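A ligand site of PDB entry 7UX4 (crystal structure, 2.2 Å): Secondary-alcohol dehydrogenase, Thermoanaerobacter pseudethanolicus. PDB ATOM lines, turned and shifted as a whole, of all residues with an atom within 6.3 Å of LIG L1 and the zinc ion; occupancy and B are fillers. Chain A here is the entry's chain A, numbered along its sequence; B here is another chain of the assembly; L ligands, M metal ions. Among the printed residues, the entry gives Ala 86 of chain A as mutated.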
ATOM      1  N   ALA A  35     -27.620   5.029 -11.780  1.00  0.00           N
ATOM      2  CA  ALA A  35     -26.664   4.648 -10.768  1.00  0.00           C
ATOM      3  C   ALA A  35     -25.490   3.916 -11.407  1.00  0.00           C
ATOM      4  O   ALA A  35     -25.718   3.054 -12.277  1.00  0.00           O
ATOM      5  CB  ALA A  35     -27.310   3.756  -9.710  1.00  0.00           C
ATOM      6  N   PRO A  36     -24.261   4.240 -11.037  1.00  0.00           N
ATOM      7  CA  PRO A  36     -23.111   3.479 -11.514  1.00  0.00           C
ATOM      8  C   PRO A  36     -22.900   2.207 -10.700  1.00  0.00           C
ATOM      9  O   PRO A  36     -23.365   2.082  -9.568  1.00  0.00           O
ATOM     10  CB  PRO A  36     -21.951   4.454 -11.323  1.00  0.00           C
ATOM     11  CG  PRO A  36     -22.349   5.243 -10.125  1.00  0.00           C
ATOM     12  CD  PRO A  36     -23.855   5.372 -10.183  1.00  0.00           C
ATOM     13  N   CYS A  37     -22.180   1.270 -11.297  1.00  0.00           N
ATOM     14  CA  CYS A  37     -21.919  -0.024 -10.677  1.00  0.00           C
ATOM     15  C   CYS A  37     -20.429  -0.332 -10.775  1.00  0.00           C
ATOM     16  O   CYS A  37     -19.688   0.278 -11.542  1.00  0.00           O
ATOM     17  CB  CYS A  37     -22.718  -1.158 -11.330  1.00  0.00           C
ATOM     18  SG  CYS A  37     -22.436  -2.793 -10.583  1.00  0.00           S
ATOM     19  N   THR A  38     -20.007  -1.317  -9.971  1.00  0.00           N
ATOM     20  CA  THR A  38     -18.634  -1.812 -10.084  1.00  0.00           C
ATOM     21  C   THR A  38     -18.368  -2.352 -11.485  1.00  0.00           C
ATOM     22  O   THR A  38     -17.225  -2.296 -11.959  1.00  0.00           O
ATOM     23  CB  THR A  38     -18.382  -2.891  -9.034  1.00  0.00           C
ATOM     24  OG1 THR A  38     -19.407  -3.884  -9.104  1.00  0.00           O
ATOM     25  CG2 THR A  38     -18.349  -2.295  -7.643  1.00  0.00           C
ATOM     26  N   SER A  39     -19.396  -2.873 -12.146  1.00  0.00           N
ATOM     27  CA  SER A  39     -19.232  -3.380 -13.500  1.00  0.00           C
ATOM     28  C   SER A  39     -18.820  -2.259 -14.455  1.00  0.00           C
ATOM     29  O   SER A  39     -17.988  -2.483 -15.356  1.00  0.00           O
ATOM     30  CB  SER A  39     -20.533  -4.038 -13.976  1.00  0.00           C
ATOM     31  OG  SER A  39     -20.866  -5.132 -13.126  1.00  0.00           O
ATOM     32  N   ASP A  40     -19.378  -1.068 -14.289  1.00  0.00           N
ATOM     33  CA  ASP A  40     -18.961   0.062 -15.106  1.00  0.00           C
ATOM     34  C   ASP A  40     -17.479   0.371 -14.903  1.00  0.00           C
ATOM     35  O   ASP A  40     -16.780   0.751 -15.859  1.00  0.00           O
ATOM     36  CB  ASP A  40     -19.804   1.308 -14.780  1.00  0.00           C
ATOM     37  CG  ASP A  40     -21.250   1.160 -15.198  1.00  0.00           C
ATOM     38  OD1 ASP A  40     -21.508   0.594 -16.286  1.00  0.00           O
ATOM     39  OD2 ASP A  40     -22.142   1.615 -14.446  1.00  0.00           O
ATOM     40  N   HIS A  59     -25.924   1.053 -16.776  1.00  0.00           N
ATOM     41  CA  HIS A  59     -26.955   0.077 -17.113  1.00  0.00           C
ATOM     42  C   HIS A  59     -28.051  -0.012 -16.052  1.00  0.00           C
ATOM     43  O   HIS A  59     -28.907  -0.888 -16.142  1.00  0.00           O
ATOM     44  CB  HIS A  59     -26.325  -1.304 -17.329  1.00  0.00           C
ATOM     45  CG  HIS A  59     -25.371  -1.701 -16.246  1.00  0.00           C
ATOM     46  ND1 HIS A  59     -24.000  -1.594 -16.396  1.00  0.00           N
ATOM     47  CD2 HIS A  59     -25.582  -2.197 -15.007  1.00  0.00           C
ATOM     48  CE1 HIS A  59     -23.412  -2.013 -15.286  1.00  0.00           C
ATOM     49  NE2 HIS A  59     -24.352  -2.376 -14.432  1.00  0.00           N
ATOM     50  N   GLU A  60     -28.057   0.876 -15.062  1.00  0.00           N
ATOM     51  CA  GLU A  60     -29.092   0.925 -14.033  1.00  0.00           C
ATOM     52  C   GLU A  60     -29.782   2.267 -14.149  1.00  0.00           C
ATOM     53  O   GLU A  60     -29.188   3.310 -13.824  1.00  0.00           O
ATOM     54  CB  GLU A  60     -28.503   0.738 -12.639  1.00  0.00           C
ATOM     55  CG  GLU A  60     -27.519  -0.407 -12.515  1.00  0.00           C
ATOM     56  CD  GLU A  60     -26.959  -0.529 -11.116  1.00  0.00           C
ATOM     57  OE1 GLU A  60     -27.619  -0.072 -10.161  1.00  0.00           O
ATOM     58  OE2 GLU A  60     -25.857  -1.097 -10.962  1.00  0.00           O
ATOM     59  N   ALA A  85     -31.362  -3.996 -16.160  1.00  0.00           N
ATOM     60  CA  ALA A  85     -30.014  -3.988 -16.715  1.00  0.00           C
ATOM     61  C   ALA A  85     -29.861  -4.999 -17.843  1.00  0.00           C
ATOM     62  O   ALA A  85     -29.097  -4.750 -18.788  1.00  0.00           O
ATOM     63  CB  ALA A  85     -28.991  -4.280 -15.606  1.00  0.00           C
ATOM     64  N   ALA A  86     -30.578  -6.121 -17.775  1.00  0.00           N
ATOM     65  CA  ALA A  86     -30.549  -7.135 -18.820  1.00  0.00           C
ATOM     66  C   ALA A  86     -31.807  -7.006 -19.678  1.00  0.00           C
ATOM     67  O   ALA A  86     -32.923  -7.233 -19.199  1.00  0.00           O
ATOM     68  CB  ALA A  86     -30.461  -8.534 -18.209  1.00  0.00           C
ATOM     69  N   LEU A 107     -24.170 -14.667 -21.633  1.00  0.00           N
ATOM     70  CA  LEU A 107     -24.352 -13.320 -21.094  1.00  0.00           C
ATOM     71  C   LEU A 107     -24.900 -12.324 -22.112  1.00  0.00           C
ATOM     72  O   LEU A 107     -24.901 -11.111 -21.858  1.00  0.00           O
ATOM     73  CB  LEU A 107     -23.067 -12.765 -20.469  1.00  0.00           C
ATOM     74  CG  LEU A 107     -22.307 -13.634 -19.472  1.00  0.00           C
ATOM     75  CD1 LEU A 107     -21.059 -12.927 -18.986  1.00  0.00           C
ATOM     76  CD2 LEU A 107     -23.206 -14.012 -18.298  1.00  0.00           C
ATOM     77  N   TRP A 110     -27.359  -9.224 -21.476  1.00  0.00           N
ATOM     78  CA  TRP A 110     -26.909  -7.929 -20.989  1.00  0.00           C
ATOM     79  C   TRP A 110     -26.350  -7.124 -22.155  1.00  0.00           C
ATOM     80  O   TRP A 110     -25.269  -7.426 -22.681  1.00  0.00           O
ATOM     81  CB  TRP A 110     -25.852  -8.103 -19.894  1.00  0.00           C
ATOM     82  CG  TRP A 110     -25.105  -6.855 -19.571  1.00  0.00           C
ATOM     83  CD1 TRP A 110     -25.623  -5.620 -19.324  1.00  0.00           C
ATOM     84  CD2 TRP A 110     -23.676  -6.711 -19.453  1.00  0.00           C
ATOM     85  NE1 TRP A 110     -24.617  -4.714 -19.067  1.00  0.00           N
ATOM     86  CE2 TRP A 110     -23.411  -5.364 -19.145  1.00  0.00           C
ATOM     87  CE3 TRP A 110     -22.613  -7.604 -19.590  1.00  0.00           C
ATOM     88  CZ2 TRP A 110     -22.120  -4.883 -18.954  1.00  0.00           C
ATOM     89  CZ3 TRP A 110     -21.322  -7.126 -19.408  1.00  0.00           C
ATOM     90  CH2 TRP A 110     -21.088  -5.779 -19.090  1.00  0.00           C
ATOM     91  N   ASP A 150     -30.605  -3.719 -11.256  1.00  0.00           N
ATOM     92  CA  ASP A 150     -29.426  -4.583 -11.194  1.00  0.00           C
ATOM     93  C   ASP A 150     -29.186  -5.132  -9.787  1.00  0.00           C
ATOM     94  O   ASP A 150     -29.104  -6.347  -9.606  1.00  0.00           O
ATOM     95  CB  ASP A 150     -28.189  -3.836 -11.674  1.00  0.00           C
ATOM     96  CG  ASP A 150     -26.983  -4.756 -11.848  1.00  0.00           C
ATOM     97  OD1 ASP A 150     -27.157  -5.990 -11.788  1.00  0.00           O
ATOM     98  OD2 ASP A 150     -25.866  -4.242 -12.044  1.00  0.00           O
ATOM     99  N   MET A 151     -29.056  -4.236  -8.805  1.00  0.00           N
ATOM    100  CA  MET A 151     -28.672  -4.672  -7.470  1.00  0.00           C
ATOM    101  C   MET A 151     -29.698  -5.633  -6.874  1.00  0.00           C
ATOM    102  O   MET A 151     -29.339  -6.690  -6.346  1.00  0.00           O
ATOM    103  CB  MET A 151     -28.473  -3.458  -6.561  1.00  0.00           C
ATOM    104  CG  MET A 151     -27.451  -2.459  -7.064  1.00  0.00           C
ATOM    105  SD  MET A 151     -25.763  -3.094  -7.118  1.00  0.00           S
ATOM    106  CE  MET A 151     -25.591  -3.572  -8.839  1.00  0.00           C
ATOM    107  N   THR A 154     -30.021  -9.034  -8.934  1.00  0.00           N
ATOM    108  CA  THR A 154     -28.838  -9.880  -8.794  1.00  0.00           C
ATOM    109  C   THR A 154     -28.822 -10.553  -7.420  1.00  0.00           C
ATOM    110  O   THR A 154     -28.743 -11.778  -7.321  1.00  0.00           O
ATOM    111  CB  THR A 154     -27.560  -9.059  -8.978  1.00  0.00           C
ATOM    112  OG1 THR A 154     -27.575  -8.443 -10.274  1.00  0.00           O
ATOM    113  CG2 THR A 154     -26.329  -9.934  -8.856  1.00  0.00           C
ATOM    114  N   TYR A 267     -18.876 -11.666  -9.857  1.00  0.00           N
ATOM    115  CA  TYR A 267     -18.181 -11.611 -11.136  1.00  0.00           C
ATOM    116  C   TYR A 267     -16.683 -11.775 -10.891  1.00  0.00           C
ATOM    117  O   TYR A 267     -16.026 -10.867 -10.369  1.00  0.00           O
ATOM    118  CB  TYR A 267     -18.487 -10.286 -11.845  1.00  0.00           C
ATOM    119  CG  TYR A 267     -17.631  -9.988 -13.054  1.00  0.00           C
ATOM    120  CD1 TYR A 267     -17.295 -10.976 -13.958  1.00  0.00           C
ATOM    121  CD2 TYR A 267     -17.168  -8.694 -13.289  1.00  0.00           C
ATOM    122  CE1 TYR A 267     -16.506 -10.699 -15.064  1.00  0.00           C
ATOM    123  CE2 TYR A 267     -16.387  -8.402 -14.390  1.00  0.00           C
ATOM    124  CZ  TYR A 267     -16.058  -9.413 -15.275  1.00  0.00           C
ATOM    125  OH  TYR A 267     -15.278  -9.118 -16.367  1.00  0.00           O
ATOM    126  N   LEU A 294     -26.064 -15.182 -14.236  1.00  0.00           N
ATOM    127  CA  LEU A 294     -26.314 -13.773 -14.502  1.00  0.00           C
ATOM    128  C   LEU A 294     -27.705 -13.395 -13.998  1.00  0.00           C
ATOM    129  O   LEU A 294     -28.634 -14.209 -13.976  1.00  0.00           O
ATOM    130  CB  LEU A 294     -26.217 -13.497 -16.003  1.00  0.00           C
ATOM    131  CG  LEU A 294     -26.201 -12.046 -16.448  1.00  0.00           C
ATOM    132  CD1 LEU A 294     -24.839 -11.458 -16.167  1.00  0.00           C
ATOM    133  CD2 LEU A 294     -26.528 -11.935 -17.930  1.00  0.00           C
ATOM    134  N   CYS A 295     -27.846 -12.134 -13.596  1.00  0.00           N
ATOM    135  CA  CYS A 295     -29.099 -11.682 -13.019  1.00  0.00           C
ATOM    136  C   CYS A 295     -30.215 -11.726 -14.060  1.00  0.00           C
ATOM    137  O   CYS A 295     -29.982 -11.454 -15.240  1.00  0.00           O
ATOM    138  CB  CYS A 295     -28.971 -10.261 -12.465  1.00  0.00           C
ATOM    139  SG  CYS A 295     -28.729  -8.988 -13.726  1.00  0.00           S
ATOM    140  N   LYS A 346     -24.119   2.799  -2.516  1.00  0.00           N
ATOM    141  CA  LYS A 346     -24.546   2.986  -3.893  1.00  0.00           C
ATOM    142  C   LYS A 346     -24.904   4.455  -4.101  1.00  0.00           C
ATOM    143  O   LYS A 346     -25.726   4.999  -3.361  1.00  0.00           O
ATOM    144  CB  LYS A 346     -25.753   2.079  -4.189  1.00  0.00           C
ATOM    145  CG  LYS A 346     -26.006   1.829  -5.674  1.00  0.00           C
ATOM    146  CD  LYS A 346     -24.975   0.870  -6.249  1.00  0.00           C
ATOM    147  CE  LYS A 346     -25.321   0.487  -7.684  1.00  0.00           C
ATOM    148  NZ  LYS A 346     -24.271  -0.391  -8.291  1.00  0.00           N
ATOM    149  N   MET B 285     -21.268 -16.637 -14.084  1.00  0.00           N
ATOM    150  CA  MET B 285     -22.633 -16.234 -14.366  1.00  0.00           C
ATOM    151  C   MET B 285     -23.220 -16.940 -15.593  1.00  0.00           C
ATOM    152  O   MET B 285     -24.152 -16.410 -16.211  1.00  0.00           O
ATOM    153  CB  MET B 285     -22.692 -14.698 -14.557  1.00  0.00           C
ATOM    154  CG  MET B 285     -22.277 -13.907 -13.306  1.00  0.00           C
ATOM    155  SD  MET B 285     -22.018 -12.144 -13.566  1.00  0.00           S
ATOM    156  CE  MET B 285     -20.740 -12.129 -14.816  1.00  0.00           C
HETATM  157  C1  LIG L   1     -24.276  -6.195 -14.127  1.00  0.00           C
HETATM  158  C2  LIG L   1     -23.006  -6.919 -14.604  1.00  0.00           C
HETATM  159  C3  LIG L   1     -23.126  -7.451 -16.024  1.00  0.00           C
HETATM  160  C4  LIG L   1     -22.092  -8.580 -16.218  1.00  0.00           C
HETATM  161  C5  LIG L   1     -24.542  -7.989 -16.295  1.00  0.00           C
HETATM  162  C6  LIG L   1     -25.631  -6.920 -16.176  1.00  0.00           C
HETATM  163  C7  LIG L   1     -25.230  -5.771 -15.254  1.00  0.00           C
HETATM  164  O1  LIG L   1     -23.883  -5.044 -13.400  1.00  0.00           O
HETATM  165  P1  LG2 L   2     -18.642  -4.633  -3.947  1.00  0.00           P
HETATM  166  O1  LG2 L   2     -17.484  -4.820  -4.862  1.00  0.00           O
HETATM  167  O2  LG2 L   2     -18.327  -3.597  -2.918  1.00  0.00           O
HETATM  168  O3  LG2 L   2     -18.939  -6.111  -3.157  1.00  0.00           O
HETATM  169  C1  LG2 L   2     -17.783  -6.834  -2.668  1.00  0.00           C
HETATM  170  C2  LG2 L   2     -18.072  -7.348  -1.241  1.00  0.00           C
HETATM  171  O4  LG2 L   2     -17.309  -8.384  -0.975  1.00  0.00           O
HETATM  172  C3  LG2 L   2     -17.641  -6.266  -0.247  1.00  0.00           C
HETATM  173  O5  LG2 L   2     -18.274  -6.425   0.947  1.00  0.00           O
HETATM  174  C4  LG2 L   2     -16.144  -6.599  -0.097  1.00  0.00           C
HETATM  175  O6  LG2 L   2     -15.579  -5.867   1.098  1.00  0.00           O
HETATM  176  C5  LG2 L   2     -16.220  -7.882   0.095  1.00  0.00           C
HETATM  177  N1  LG2 L   2     -14.929  -8.560  -0.141  1.00  0.00           N
HETATM  178  C6  LG2 L   2     -13.825  -8.272  -0.861  1.00  0.00           C
HETATM  179  N2  LG2 L   2     -12.964  -9.281  -0.689  1.00  0.00           N
HETATM  180  C7  LG2 L   2     -13.523 -10.190   0.131  1.00  0.00           C
HETATM  181  C8  LG2 L   2     -13.080 -11.406   0.640  1.00  0.00           C
HETATM  182  N3  LG2 L   2     -11.775 -12.188   0.457  1.00  0.00           N
HETATM  183  N4  LG2 L   2     -13.842 -12.097   1.439  1.00  0.00           N
HETATM  184  C9  LG2 L   2     -15.096 -11.637   1.787  1.00  0.00           C
HETATM  185  N5  LG2 L   2     -15.526 -10.448   1.300  1.00  0.00           N
HETATM  186  C10 LG2 L   2     -14.738  -9.741   0.473  1.00  0.00           C
HETATM  187  O7  LG2 L   2     -19.966  -4.166  -4.825  1.00  0.00           O
HETATM  188  P2  LG2 L   2     -21.073  -5.244  -5.469  1.00  0.00           P
HETATM  189  O8  LG2 L   2     -21.874  -4.557  -6.588  1.00  0.00           O
HETATM  190  O9  LG2 L   2     -22.063  -5.714  -4.359  1.00  0.00           O
HETATM  191  O10 LG2 L   2     -20.221  -6.549  -6.052  1.00  0.00           O
HETATM  192  C11 LG2 L   2     -20.886  -7.759  -6.313  1.00  0.00           C
HETATM  193  C12 LG2 L   2     -20.050  -8.579  -7.352  1.00  0.00           C
HETATM  194  O11 LG2 L   2     -20.851  -9.202  -8.190  1.00  0.00           O
HETATM  195  C13 LG2 L   2     -19.175  -7.648  -8.201  1.00  0.00           C
HETATM  196  O12 LG2 L   2     -18.016  -8.262  -8.522  1.00  0.00           O
HETATM  197  C14 LG2 L   2     -20.033  -7.389  -9.462  1.00  0.00           C
HETATM  198  O13 LG2 L   2     -19.157  -7.091 -10.659  1.00  0.00           O
HETATM  199  C15 LG2 L   2     -20.691  -8.512  -9.638  1.00  0.00           C
HETATM  200  N6  LG2 L   2     -22.028  -8.288 -10.192  1.00  0.00           N
HETATM  201  C16 LG2 L   2     -22.696  -9.339 -10.776  1.00  0.00           C
HETATM  202  C17 LG2 L   2     -23.981  -9.150 -11.303  1.00  0.00           C
HETATM  203  C18 LG2 L   2     -24.756 -10.332 -11.978  1.00  0.00           C
HETATM  204  O14 LG2 L   2     -25.608 -10.105 -12.816  1.00  0.00           O
HETATM  205  N7  LG2 L   2     -24.438 -11.753 -11.618  1.00  0.00           N
HETATM  206  C19 LG2 L   2     -24.563  -7.923 -11.228  1.00  0.00           C
HETATM  207  C20 LG2 L   2     -23.895  -6.873 -10.644  1.00  0.00           C
HETATM  208  C21 LG2 L   2     -22.611  -7.074 -10.123  1.00  0.00           C
HETATM  209  P3  LG2 L   2     -15.406  -4.221   0.936  1.00  0.00           P
HETATM  210  O15 LG2 L   2     -14.132  -3.765   1.666  1.00  0.00           O
HETATM  211  O16 LG2 L   2     -16.612  -3.516   1.542  1.00  0.00           O
HETATM  212  O17 LG2 L   2     -15.298  -3.867  -0.530  1.00  0.00           O
HETATM  213 ZN    ZN M   1     -24.516  -2.703 -12.094  1.00  0.00          ZN
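OD2 of Asp 150 lies close to O1 of LIG L1, 2.5 Å away. An oxygen (O1) of LIG L1 lies close to a ring nitrogen (NE2) of His 59, 2.9 Å away. OG of Ser 39 sits at hydrogen-bond distance from O1 of LIG L1, 3.0 Å away. The side-chain sulfur (SD) of Met 285 of chain B is in hydrogen-bond range of a nitrogen (N7) of LG2 L2 (3.1 Å). The backbone NH (N) of Cys 295 is in hydrogen-bond range of an oxygen (O14) of LG2 L2, at 3.1 Å. The side-chain sulfur of Cys 295 lies close to an oxygen (O14) of LG2 L2.
The backbone carbonyl oxygen (O) of Asp 150 is in hydrogen-bond range of the side-chain hydroxyl (OG1) of Thr 154, 2.7 Å away. The side-chain amino group (NZ) of Lys 346 lies within salt-bridge range of the side-chain carboxylate (OE1) of Glu 60 (3.8 Å). O of Glu 60 lies within hydrogen-bond range of N of Ala 35 (3.1 Å). The side-chain sulfur of Cys 37 lies close to the backbone NH of Ser 39 (3.4 Å). The side-chain sulfur (SG) of Cys 37 sits close to the side-chain amino group (NZ) of Lys 346 (3.8 Å). OD2 of Asp 40 is in hydrogen-bond range of N of Cys 37. The backbone carbonyl oxygen (O) of Met 285 of chain B sits at hydrogen-bond distance from the backbone NH (N) of Leu 294 (3.0 Å). SD of Met 151 lies within hydrogen-bond range of NZ of Lys 346 (3.3 Å).
Merely in contact with LIG L1: Trp 110 (3.4 Å) and Leu 294 (3.5 Å). Within 4 Å of LIG L1: Cys 37, Ser 39, His 59, Trp 110, Asp 150 and Leu 294. The nearest printed residue that does not touch LIG L1 is Met 285 of chain B (4.05 Å).
CE of Met 151 touches the zinc ion (3.5 Å). Five residues have an atom within 4 Å of the zinc ion: Cys 37, His 59, Glu 60, Asp 150 and Met 151. The nearest printed residue that does not touch the zinc ion is Lys 346 (4.5 Å).
The zinc ion is bound by OD2 of Asp 150 (2.0 Å), NE2 of His 59 (2.4 Å), OE2 of Glu 60 (2.4 Å) and SG of Cys 37 (2.6 Å). Slightly farther from the zinc ion lies an oxygen (O1) of LIG L1 (2.8 Å).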
